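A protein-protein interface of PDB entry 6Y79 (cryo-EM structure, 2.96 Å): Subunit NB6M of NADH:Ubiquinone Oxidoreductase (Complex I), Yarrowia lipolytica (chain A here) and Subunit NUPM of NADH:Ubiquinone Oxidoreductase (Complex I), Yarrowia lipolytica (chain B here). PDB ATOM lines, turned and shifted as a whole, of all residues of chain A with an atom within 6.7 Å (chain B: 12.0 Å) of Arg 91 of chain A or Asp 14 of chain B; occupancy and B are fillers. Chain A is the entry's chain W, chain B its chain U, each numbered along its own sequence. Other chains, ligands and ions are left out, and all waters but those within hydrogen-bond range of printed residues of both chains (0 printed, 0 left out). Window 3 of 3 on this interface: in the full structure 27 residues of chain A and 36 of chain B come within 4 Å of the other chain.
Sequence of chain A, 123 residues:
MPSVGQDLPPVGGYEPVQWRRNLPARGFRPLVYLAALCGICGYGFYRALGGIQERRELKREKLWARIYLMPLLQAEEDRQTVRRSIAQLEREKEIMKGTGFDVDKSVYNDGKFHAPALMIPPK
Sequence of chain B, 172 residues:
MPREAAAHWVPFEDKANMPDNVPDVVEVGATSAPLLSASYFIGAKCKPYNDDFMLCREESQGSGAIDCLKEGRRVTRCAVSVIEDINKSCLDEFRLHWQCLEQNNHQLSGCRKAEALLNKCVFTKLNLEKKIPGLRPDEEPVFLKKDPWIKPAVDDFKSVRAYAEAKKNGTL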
ATOM      1  N   GLN A  80      33.147  27.985  24.183  1.00  0.00           N
ATOM      2  CA  GLN A  80      32.461  28.738  23.135  1.00  0.00           C
ATOM      3  C   GLN A  80      32.779  28.183  21.751  1.00  0.00           C
ATOM      4  O   GLN A  80      31.882  28.061  20.907  1.00  0.00           O
ATOM      5  CB  GLN A  80      32.832  30.218  23.208  1.00  0.00           C
ATOM      6  CG  GLN A  80      32.308  30.950  24.433  1.00  0.00           C
ATOM      7  CD  GLN A  80      30.802  30.888  24.567  1.00  0.00           C
ATOM      8  OE1 GLN A  80      30.070  30.955  23.581  1.00  0.00           O
ATOM      9  NE2 GLN A  80      30.329  30.758  25.797  1.00  0.00           N
ATOM     10  N   ARG A  83      30.875  24.766  21.280  1.00  0.00           N
ATOM     11  CA  ARG A  83      29.442  24.959  21.071  1.00  0.00           C
ATOM     12  C   ARG A  83      29.113  25.549  19.702  1.00  0.00           C
ATOM     13  O   ARG A  83      28.288  24.986  18.973  1.00  0.00           O
ATOM     14  CB  ARG A  83      28.881  25.842  22.173  1.00  0.00           C
ATOM     15  CG  ARG A  83      27.407  26.059  22.018  1.00  0.00           C
ATOM     16  CD  ARG A  83      26.912  27.046  23.047  1.00  0.00           C
ATOM     17  NE  ARG A  83      27.533  28.367  22.930  1.00  0.00           N
ATOM     18  CZ  ARG A  83      27.076  29.377  22.189  1.00  0.00           C
ATOM     19  NH1 ARG A  83      27.744  30.523  22.203  1.00  0.00           N
ATOM     20  NH2 ARG A  83      25.970  29.274  21.452  1.00  0.00           N
ATOM     21  N   ARG A  84      29.819  26.614  19.289  1.00  0.00           N
ATOM     22  CA  ARG A  84      29.467  27.258  18.027  1.00  0.00           C
ATOM     23  C   ARG A  84      29.860  26.415  16.822  1.00  0.00           C
ATOM     24  O   ARG A  84      29.175  26.457  15.793  1.00  0.00           O
ATOM     25  CB  ARG A  84      30.117  28.625  17.935  1.00  0.00           C
ATOM     26  CG  ARG A  84      29.733  29.548  19.055  1.00  0.00           C
ATOM     27  CD  ARG A  84      30.505  30.805  18.952  1.00  0.00           C
ATOM     28  NE  ARG A  84      30.201  31.399  17.671  1.00  0.00           N
ATOM     29  CZ  ARG A  84      29.405  32.442  17.526  1.00  0.00           C
ATOM     30  NH1 ARG A  84      29.147  32.924  16.325  1.00  0.00           N
ATOM     31  NH2 ARG A  84      28.875  33.001  18.594  1.00  0.00           N
ATOM     32  N   SER A  85      30.910  25.595  16.944  1.00  0.00           N
ATOM     33  CA  SER A  85      31.305  24.729  15.835  1.00  0.00           C
ATOM     34  C   SER A  85      30.345  23.553  15.662  1.00  0.00           C
ATOM     35  O   SER A  85      29.982  23.200  14.528  1.00  0.00           O
ATOM     36  CB  SER A  85      32.731  24.229  16.054  1.00  0.00           C
ATOM     37  OG  SER A  85      32.799  23.390  17.182  1.00  0.00           O
ATOM     38  N   ILE A  86      29.921  22.927  16.773  1.00  0.00           N
ATOM     39  CA  ILE A  86      28.911  21.870  16.681  1.00  0.00           C
ATOM     40  C   ILE A  86      27.579  22.438  16.199  1.00  0.00           C
ATOM     41  O   ILE A  86      26.847  21.778  15.445  1.00  0.00           O
ATOM     42  CB  ILE A  86      28.794  21.146  18.039  1.00  0.00           C
ATOM     43  CG1 ILE A  86      30.078  20.380  18.334  1.00  0.00           C
ATOM     44  CG2 ILE A  86      27.636  20.156  18.080  1.00  0.00           C
ATOM     45  CD1 ILE A  86      30.080  19.684  19.670  1.00  0.00           C
ATOM     46  N   ALA A  87      27.287  23.691  16.555  1.00  0.00           N
ATOM     47  CA  ALA A  87      26.096  24.371  16.062  1.00  0.00           C
ATOM     48  C   ALA A  87      26.144  24.579  14.555  1.00  0.00           C
ATOM     49  O   ALA A  87      25.150  24.351  13.858  1.00  0.00           O
ATOM     50  CB  ALA A  87      25.947  25.710  16.766  1.00  0.00           C
ATOM     51  N   GLN A  88      27.294  25.021  14.035  1.00  0.00           N
ATOM     52  CA  GLN A  88      27.447  25.207  12.592  1.00  0.00           C
ATOM     53  C   GLN A  88      27.383  23.880  11.845  1.00  0.00           C
ATOM     54  O   GLN A  88      26.814  23.801  10.746  1.00  0.00           O
ATOM     55  CB  GLN A  88      28.767  25.917  12.301  1.00  0.00           C
ATOM     56  CG  GLN A  88      29.007  26.215  10.835  1.00  0.00           C
ATOM     57  CD  GLN A  88      28.121  27.323  10.328  1.00  0.00           C
ATOM     58  OE1 GLN A  88      27.928  28.333  11.004  1.00  0.00           O
ATOM     59  NE2 GLN A  88      27.565  27.143   9.139  1.00  0.00           N
ATOM     60  N   LEU A  89      27.954  22.830  12.443  1.00  0.00           N
ATOM     61  CA  LEU A  89      27.932  21.496  11.852  1.00  0.00           C
ATOM     62  C   LEU A  89      26.511  20.965  11.731  1.00  0.00           C
ATOM     63  O   LEU A  89      26.091  20.510  10.655  1.00  0.00           O
ATOM     64  CB  LEU A  89      28.777  20.558  12.706  1.00  0.00           C
ATOM     65  CG  LEU A  89      28.842  19.108  12.257  1.00  0.00           C
ATOM     66  CD1 LEU A  89      29.644  19.018  10.988  1.00  0.00           C
ATOM     67  CD2 LEU A  89      29.455  18.256  13.345  1.00  0.00           C
ATOM     68  N   GLU A  90      25.746  21.040  12.828  1.00  0.00           N
ATOM     69  CA  GLU A  90      24.336  20.673  12.786  1.00  0.00           C
ATOM     70  C   GLU A  90      23.549  21.576  11.854  1.00  0.00           C
ATOM     71  O   GLU A  90      22.595  21.113  11.232  1.00  0.00           O
ATOM     72  CB  GLU A  90      23.720  20.715  14.185  1.00  0.00           C
ATOM     73  CG  GLU A  90      24.253  19.656  15.117  1.00  0.00           C
ATOM     74  CD  GLU A  90      23.957  18.249  14.635  1.00  0.00           C
ATOM     75  OE1 GLU A  90      22.840  18.006  14.136  1.00  0.00           O
ATOM     76  OE2 GLU A  90      24.851  17.385  14.750  1.00  0.00           O
ATOM     77  N   ARG A  91      23.944  22.846  11.723  1.00  0.00           N
ATOM     78  CA  ARG A  91      23.223  23.768  10.856  1.00  0.00           C
ATOM     79  C   ARG A  91      23.339  23.351   9.398  1.00  0.00           C
ATOM     80  O   ARG A  91      22.329  23.253   8.698  1.00  0.00           O
ATOM     81  CB  ARG A  91      23.742  25.186  11.045  1.00  0.00           C
ATOM     82  CG  ARG A  91      23.004  26.228  10.216  1.00  0.00           C
ATOM     83  CD  ARG A  91      23.231  27.629  10.757  1.00  0.00           C
ATOM     84  NE  ARG A  91      23.469  27.623  12.198  1.00  0.00           N
ATOM     85  CZ  ARG A  91      24.605  28.008  12.770  1.00  0.00           C
ATOM     86  NH1 ARG A  91      24.737  27.960  14.087  1.00  0.00           N
ATOM     87  NH2 ARG A  91      25.617  28.407  12.017  1.00  0.00           N
ATOM     88  N   GLU A  92      24.558  23.057   8.927  1.00  0.00           N
ATOM     89  CA  GLU A  92      24.669  22.646   7.528  1.00  0.00           C
ATOM     90  C   GLU A  92      24.227  21.199   7.320  1.00  0.00           C
ATOM     91  O   GLU A  92      23.964  20.803   6.178  1.00  0.00           O
ATOM     92  CB  GLU A  92      26.081  22.871   6.996  1.00  0.00           C
ATOM     93  CG  GLU A  92      27.209  22.349   7.841  1.00  0.00           C
ATOM     94  CD  GLU A  92      28.459  23.186   7.667  1.00  0.00           C
ATOM     95  OE1 GLU A  92      29.546  22.755   8.097  1.00  0.00           O
ATOM     96  OE2 GLU A  92      28.346  24.298   7.106  1.00  0.00           O
ATOM     97  N   LYS A  93      24.125  20.396   8.390  1.00  0.00           N
ATOM     98  CA  LYS A  93      23.387  19.136   8.272  1.00  0.00           C
ATOM     99  C   LYS A  93      21.896  19.390   8.057  1.00  0.00           C
ATOM    100  O   LYS A  93      21.260  18.731   7.229  1.00  0.00           O
ATOM    101  CB  LYS A  93      23.615  18.280   9.509  1.00  0.00           C
ATOM    102  CG  LYS A  93      23.060  16.874   9.420  1.00  0.00           C
ATOM    103  CD  LYS A  93      23.314  16.120  10.712  1.00  0.00           C
ATOM    104  CE  LYS A  93      24.792  15.825  10.880  1.00  0.00           C
ATOM    105  NZ  LYS A  93      25.287  14.887   9.843  1.00  0.00           N
ATOM    106  N   GLU A  94      21.325  20.355   8.787  1.00  0.00           N
ATOM    107  CA  GLU A  94      19.941  20.741   8.559  1.00  0.00           C
ATOM    108  C   GLU A  94      19.768  21.455   7.218  1.00  0.00           C
ATOM    109  O   GLU A  94      18.645  21.530   6.716  1.00  0.00           O
ATOM    110  CB  GLU A  94      19.422  21.585   9.727  1.00  0.00           C
ATOM    111  CG  GLU A  94      19.298  20.869  11.092  1.00  0.00           C
ATOM    112  CD  GLU A  94      19.761  21.784  12.253  1.00  0.00           C
ATOM    113  OE1 GLU A  94      19.700  21.364  13.418  1.00  0.00           O
ATOM    114  OE2 GLU A  94      20.188  22.920  11.939  1.00  0.00           O
ATOM    115  N   ILE A  95      20.839  21.994   6.631  1.00  0.00           N
ATOM    116  CA  ILE A  95      20.721  22.602   5.310  1.00  0.00           C
ATOM    117  C   ILE A  95      20.608  21.524   4.238  1.00  0.00           C
ATOM    118  O   ILE A  95      19.666  21.524   3.443  1.00  0.00           O
ATOM    119  CB  ILE A  95      21.892  23.566   5.034  1.00  0.00           C
ATOM    120  CG1 ILE A  95      21.787  24.830   5.896  1.00  0.00           C
ATOM    121  CG2 ILE A  95      21.959  23.925   3.547  1.00  0.00           C
ATOM    122  CD1 ILE A  95      23.012  25.706   5.843  1.00  0.00           C
ATOM    123  N   MET A  96      21.545  20.578   4.212  1.00  0.00           N
ATOM    124  CA  MET A  96      21.655  19.619   3.117  1.00  0.00           C
ATOM    125  C   MET A  96      21.019  18.273   3.430  1.00  0.00           C
ATOM    126  O   MET A  96      21.561  17.231   3.039  1.00  0.00           O
ATOM    127  CB  MET A  96      23.116  19.439   2.730  1.00  0.00           C
ATOM    128  CG  MET A  96      23.814  20.743   2.556  1.00  0.00           C
ATOM    129  SD  MET A  96      25.346  20.457   1.693  1.00  0.00           S
ATOM    130  CE  MET A  96      24.766  19.693   0.186  1.00  0.00           C
ATOM    131  N   VAL B  10      32.634  41.982  10.602  1.00  0.00           N
ATOM    132  CA  VAL B  10      31.316  42.162  11.201  1.00  0.00           C
ATOM    133  C   VAL B  10      31.054  41.058  12.212  1.00  0.00           C
ATOM    134  O   VAL B  10      31.347  39.886  11.952  1.00  0.00           O
ATOM    135  CB  VAL B  10      30.164  42.285  10.179  1.00  0.00           C
ATOM    136  CG1 VAL B  10      30.412  43.483   9.270  1.00  0.00           C
ATOM    137  CG2 VAL B  10      29.891  40.999   9.345  1.00  0.00           C
ATOM    138  N   PRO B  11      30.590  41.393  13.415  1.00  0.00           N
ATOM    139  CA  PRO B  11      30.465  40.391  14.475  1.00  0.00           C
ATOM    140  C   PRO B  11      29.189  39.579  14.352  1.00  0.00           C
ATOM    141  O   PRO B  11      28.162  40.054  13.865  1.00  0.00           O
ATOM    142  CB  PRO B  11      30.475  41.230  15.757  1.00  0.00           C
ATOM    143  CG  PRO B  11      30.063  42.579  15.345  1.00  0.00           C
ATOM    144  CD  PRO B  11      30.406  42.768  13.913  1.00  0.00           C
ATOM    145  N   PHE B  12      29.265  38.333  14.795  1.00  0.00           N
ATOM    146  CA  PHE B  12      28.115  37.453  14.689  1.00  0.00           C
ATOM    147  C   PHE B  12      28.093  36.478  15.850  1.00  0.00           C
ATOM    148  O   PHE B  12      29.142  36.037  16.327  1.00  0.00           O
ATOM    149  CB  PHE B  12      28.081  36.692  13.348  1.00  0.00           C
ATOM    150  CG  PHE B  12      29.163  35.674  13.187  1.00  0.00           C
ATOM    151  CD1 PHE B  12      30.433  36.059  12.812  1.00  0.00           C
ATOM    152  CD2 PHE B  12      28.904  34.327  13.375  1.00  0.00           C
ATOM    153  CE1 PHE B  12      31.429  35.130  12.658  1.00  0.00           C
ATOM    154  CE2 PHE B  12      29.904  33.392  13.218  1.00  0.00           C
ATOM    155  CZ  PHE B  12      31.164  33.795  12.868  1.00  0.00           C
ATOM    156  N   GLU B  13      26.892  36.148  16.300  1.00  0.00           N
ATOM    157  CA  GLU B  13      26.734  35.242  17.417  1.00  0.00           C
ATOM    158  C   GLU B  13      25.766  34.127  17.079  1.00  0.00           C
ATOM    159  O   GLU B  13      25.128  34.125  16.028  1.00  0.00           O
ATOM    160  CB  GLU B  13      26.277  35.977  18.666  1.00  0.00           C
ATOM    161  CG  GLU B  13      24.913  36.489  18.668  1.00  0.00           C
ATOM    162  CD  GLU B  13      24.783  37.917  18.153  1.00  0.00           C
ATOM    163  OE1 GLU B  13      25.625  38.390  17.372  1.00  0.00           O
ATOM    164  OE2 GLU B  13      23.893  38.596  18.681  1.00  0.00           O
ATOM    165  N   ASP B  14      25.642  33.192  18.012  1.00  0.00           N
ATOM    166  CA  ASP B  14      25.135  31.871  17.683  1.00  0.00           C
ATOM    167  C   ASP B  14      24.059  31.446  18.673  1.00  0.00           C
ATOM    168  O   ASP B  14      24.332  31.253  19.865  1.00  0.00           O
ATOM    169  CB  ASP B  14      26.281  30.871  17.646  1.00  0.00           C
ATOM    170  CG  ASP B  14      25.813  29.489  17.331  1.00  0.00           C
ATOM    171  OD1 ASP B  14      25.393  29.229  16.184  1.00  0.00           O
ATOM    172  OD2 ASP B  14      25.907  28.650  18.236  1.00  0.00           O
ATOM    173  N   LYS B  15      22.844  31.289  18.159  1.00  0.00           N
ATOM    174  CA  LYS B  15      21.715  30.864  18.976  1.00  0.00           C
ATOM    175  C   LYS B  15      21.750  29.378  19.248  1.00  0.00           C
ATOM    176  O   LYS B  15      20.936  28.646  18.692  1.00  0.00           O
ATOM    177  CB  LYS B  15      20.396  31.162  18.284  1.00  0.00           C
ATOM    178  CG  LYS B  15      19.838  32.495  18.468  1.00  0.00           C
ATOM    179  CD  LYS B  15      20.207  33.399  17.327  1.00  0.00           C
ATOM    180  CE  LYS B  15      19.210  34.539  17.349  1.00  0.00           C
ATOM    181  NZ  LYS B  15      19.311  35.527  16.231  1.00  0.00           N
ATOM    182  N   ALA B  16      22.609  28.905  20.147  1.00  0.00           N
ATOM    183  CA  ALA B  16      22.622  27.466  20.331  1.00  0.00           C
ATOM    184  C   ALA B  16      22.994  27.097  21.745  1.00  0.00           C
ATOM    185  O   ALA B  16      23.132  27.947  22.621  1.00  0.00           O
ATOM    186  CB  ALA B  16      23.553  26.785  19.353  1.00  0.00           C
ATOM    187  N   ASN B  17      23.170  25.804  21.941  1.00  0.00           N
ATOM    188  CA  ASN B  17      23.383  25.236  23.254  1.00  0.00           C
ATOM    189  C   ASN B  17      24.500  24.205  23.202  1.00  0.00           C
ATOM    190  O   ASN B  17      24.803  23.650  22.139  1.00  0.00           O
ATOM    191  CB  ASN B  17      22.102  24.573  23.783  1.00  0.00           C
ATOM    192  CG  ASN B  17      21.016  25.575  24.113  1.00  0.00           C
ATOM    193  OD1 ASN B  17      21.281  26.620  24.700  1.00  0.00           O
ATOM    194  ND2 ASN B  17      19.785  25.262  23.735  1.00  0.00           N
ATOM    195  N   MET B  18      25.111  23.984  24.371  1.00  0.00           N
ATOM    196  CA  MET B  18      25.892  22.784  24.632  1.00  0.00           C
ATOM    197  C   MET B  18      25.070  21.541  24.299  1.00  0.00           C
ATOM    198  O   MET B  18      23.866  21.497  24.580  1.00  0.00           O
ATOM    199  CB  MET B  18      26.280  22.672  26.108  1.00  0.00           C
ATOM    200  CG  MET B  18      27.299  23.632  26.736  1.00  0.00           C
ATOM    201  SD  MET B  18      28.961  23.734  26.017  1.00  0.00           S
ATOM    202  CE  MET B  18      29.295  25.508  25.800  1.00  0.00           C
ATOM    203  N   PRO B  19      25.687  20.496  23.768  1.00  0.00           N
ATOM    204  CA  PRO B  19      24.991  19.204  23.685  1.00  0.00           C
ATOM    205  C   PRO B  19      24.821  18.543  25.052  1.00  0.00           C
ATOM    206  O   PRO B  19      25.334  19.031  26.065  1.00  0.00           O
ATOM    207  CB  PRO B  19      25.904  18.384  22.766  1.00  0.00           C
ATOM    208  CG  PRO B  19      27.258  18.976  22.968  1.00  0.00           C
ATOM    209  CD  PRO B  19      27.020  20.445  23.146  1.00  0.00           C
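O of Phe 12 of chain B is in hydrogen-bond range of NH1 of Arg 84 of chain A, 3.1 Å away.
OD2 of Asp 14 of chain B is in salt-bridge range of NH2 of Arg 83 of chain A (3.3 Å).
OD1 of Asp 14 of chain B is in salt-bridge range of NH1 of Arg 91 of chain A (2.5 Å).
O of Ala 16 of chain B sits at hydrogen-bond distance from NH2 of Arg 83 of chain A (3.3 Å).
N of Asp 14 of chain B sits close to NH2 of Arg 84 of chain A (3.3 Å).
OE1 of Gln 80 of chain A is in hydrogen-bond range of NH1 of Arg 83 of chain A (2.7 Å).
OE1 of Gln 88 of chain A sits at hydrogen-bond distance from NH2 of Arg 91 of chain A, at 2.5 Å.
O of Asn 17 of chain B touches CG of Arg 83 of chain A (3.5 Å).
Arg 83 of chain A touches Met 18 of chain B.
Arg 84 of chain A touches Glu 13 of chain B.
Ala 87 of chain A touches Asp 14 of chain B.
CB of Ala 87 of chain A touches CB of Ala 16 of chain B, at 3.7 Å.
Ser 85 of chain A touches none of the printed residues of chain B.
Of chain B, only Asp 14 (3.3 Å) and Ala 16 (3.7 Å) come within 4 Å of Ala 87 of chain A.
No residue of chain B comes within 4 Å of Gln 88 of chain A.
No residue of chain B comes within 4 Å of Leu 89 of chain A.
Of chain B, only Asp 14 (2.5 Å) comes within 4 Å of Arg 91 of chain A.
No residue of chain B comes within 4 Å of Glu 92 of chain A.
Glu 94 of chain A touches none of the printed residues of chain B.
No residue of chain B comes within 4 Å of Ile 95 of chain A.
Pro 11 of chain B touches none of the printed residues of chain A.
Printed residues of chain A within 4 Å of Phe 12 of chain B: Arg 84 (3.1 Å).
Of the printed residues of chain A, Glu 13 of chain B touches Arg 84.
Of chain A, only Arg 83, Arg 84, Ala 87 and Arg 91 come within 4 Å of Asp 14 of chain B.
Printed residues of chain A within 4 Å of Asn 17 of chain B: Arg 83.
Printed residues of chain A within 4 Å of Met 18 of chain B: Arg 83 (3.7 Å).
Along chain A the printed residues that touch a printed residue of chain B span positions 83 to 91.
Among the printed residues, 10 pairs touch across the chains.
Among the printed residues, Asp or Glu carboxylates within 4 Å of a Lys or Arg side-chain nitrogen of the other chain: Arg 83 of chain A with Asp 14 of chain B and Arg 91 of chain A with Asp 14 of chain B.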
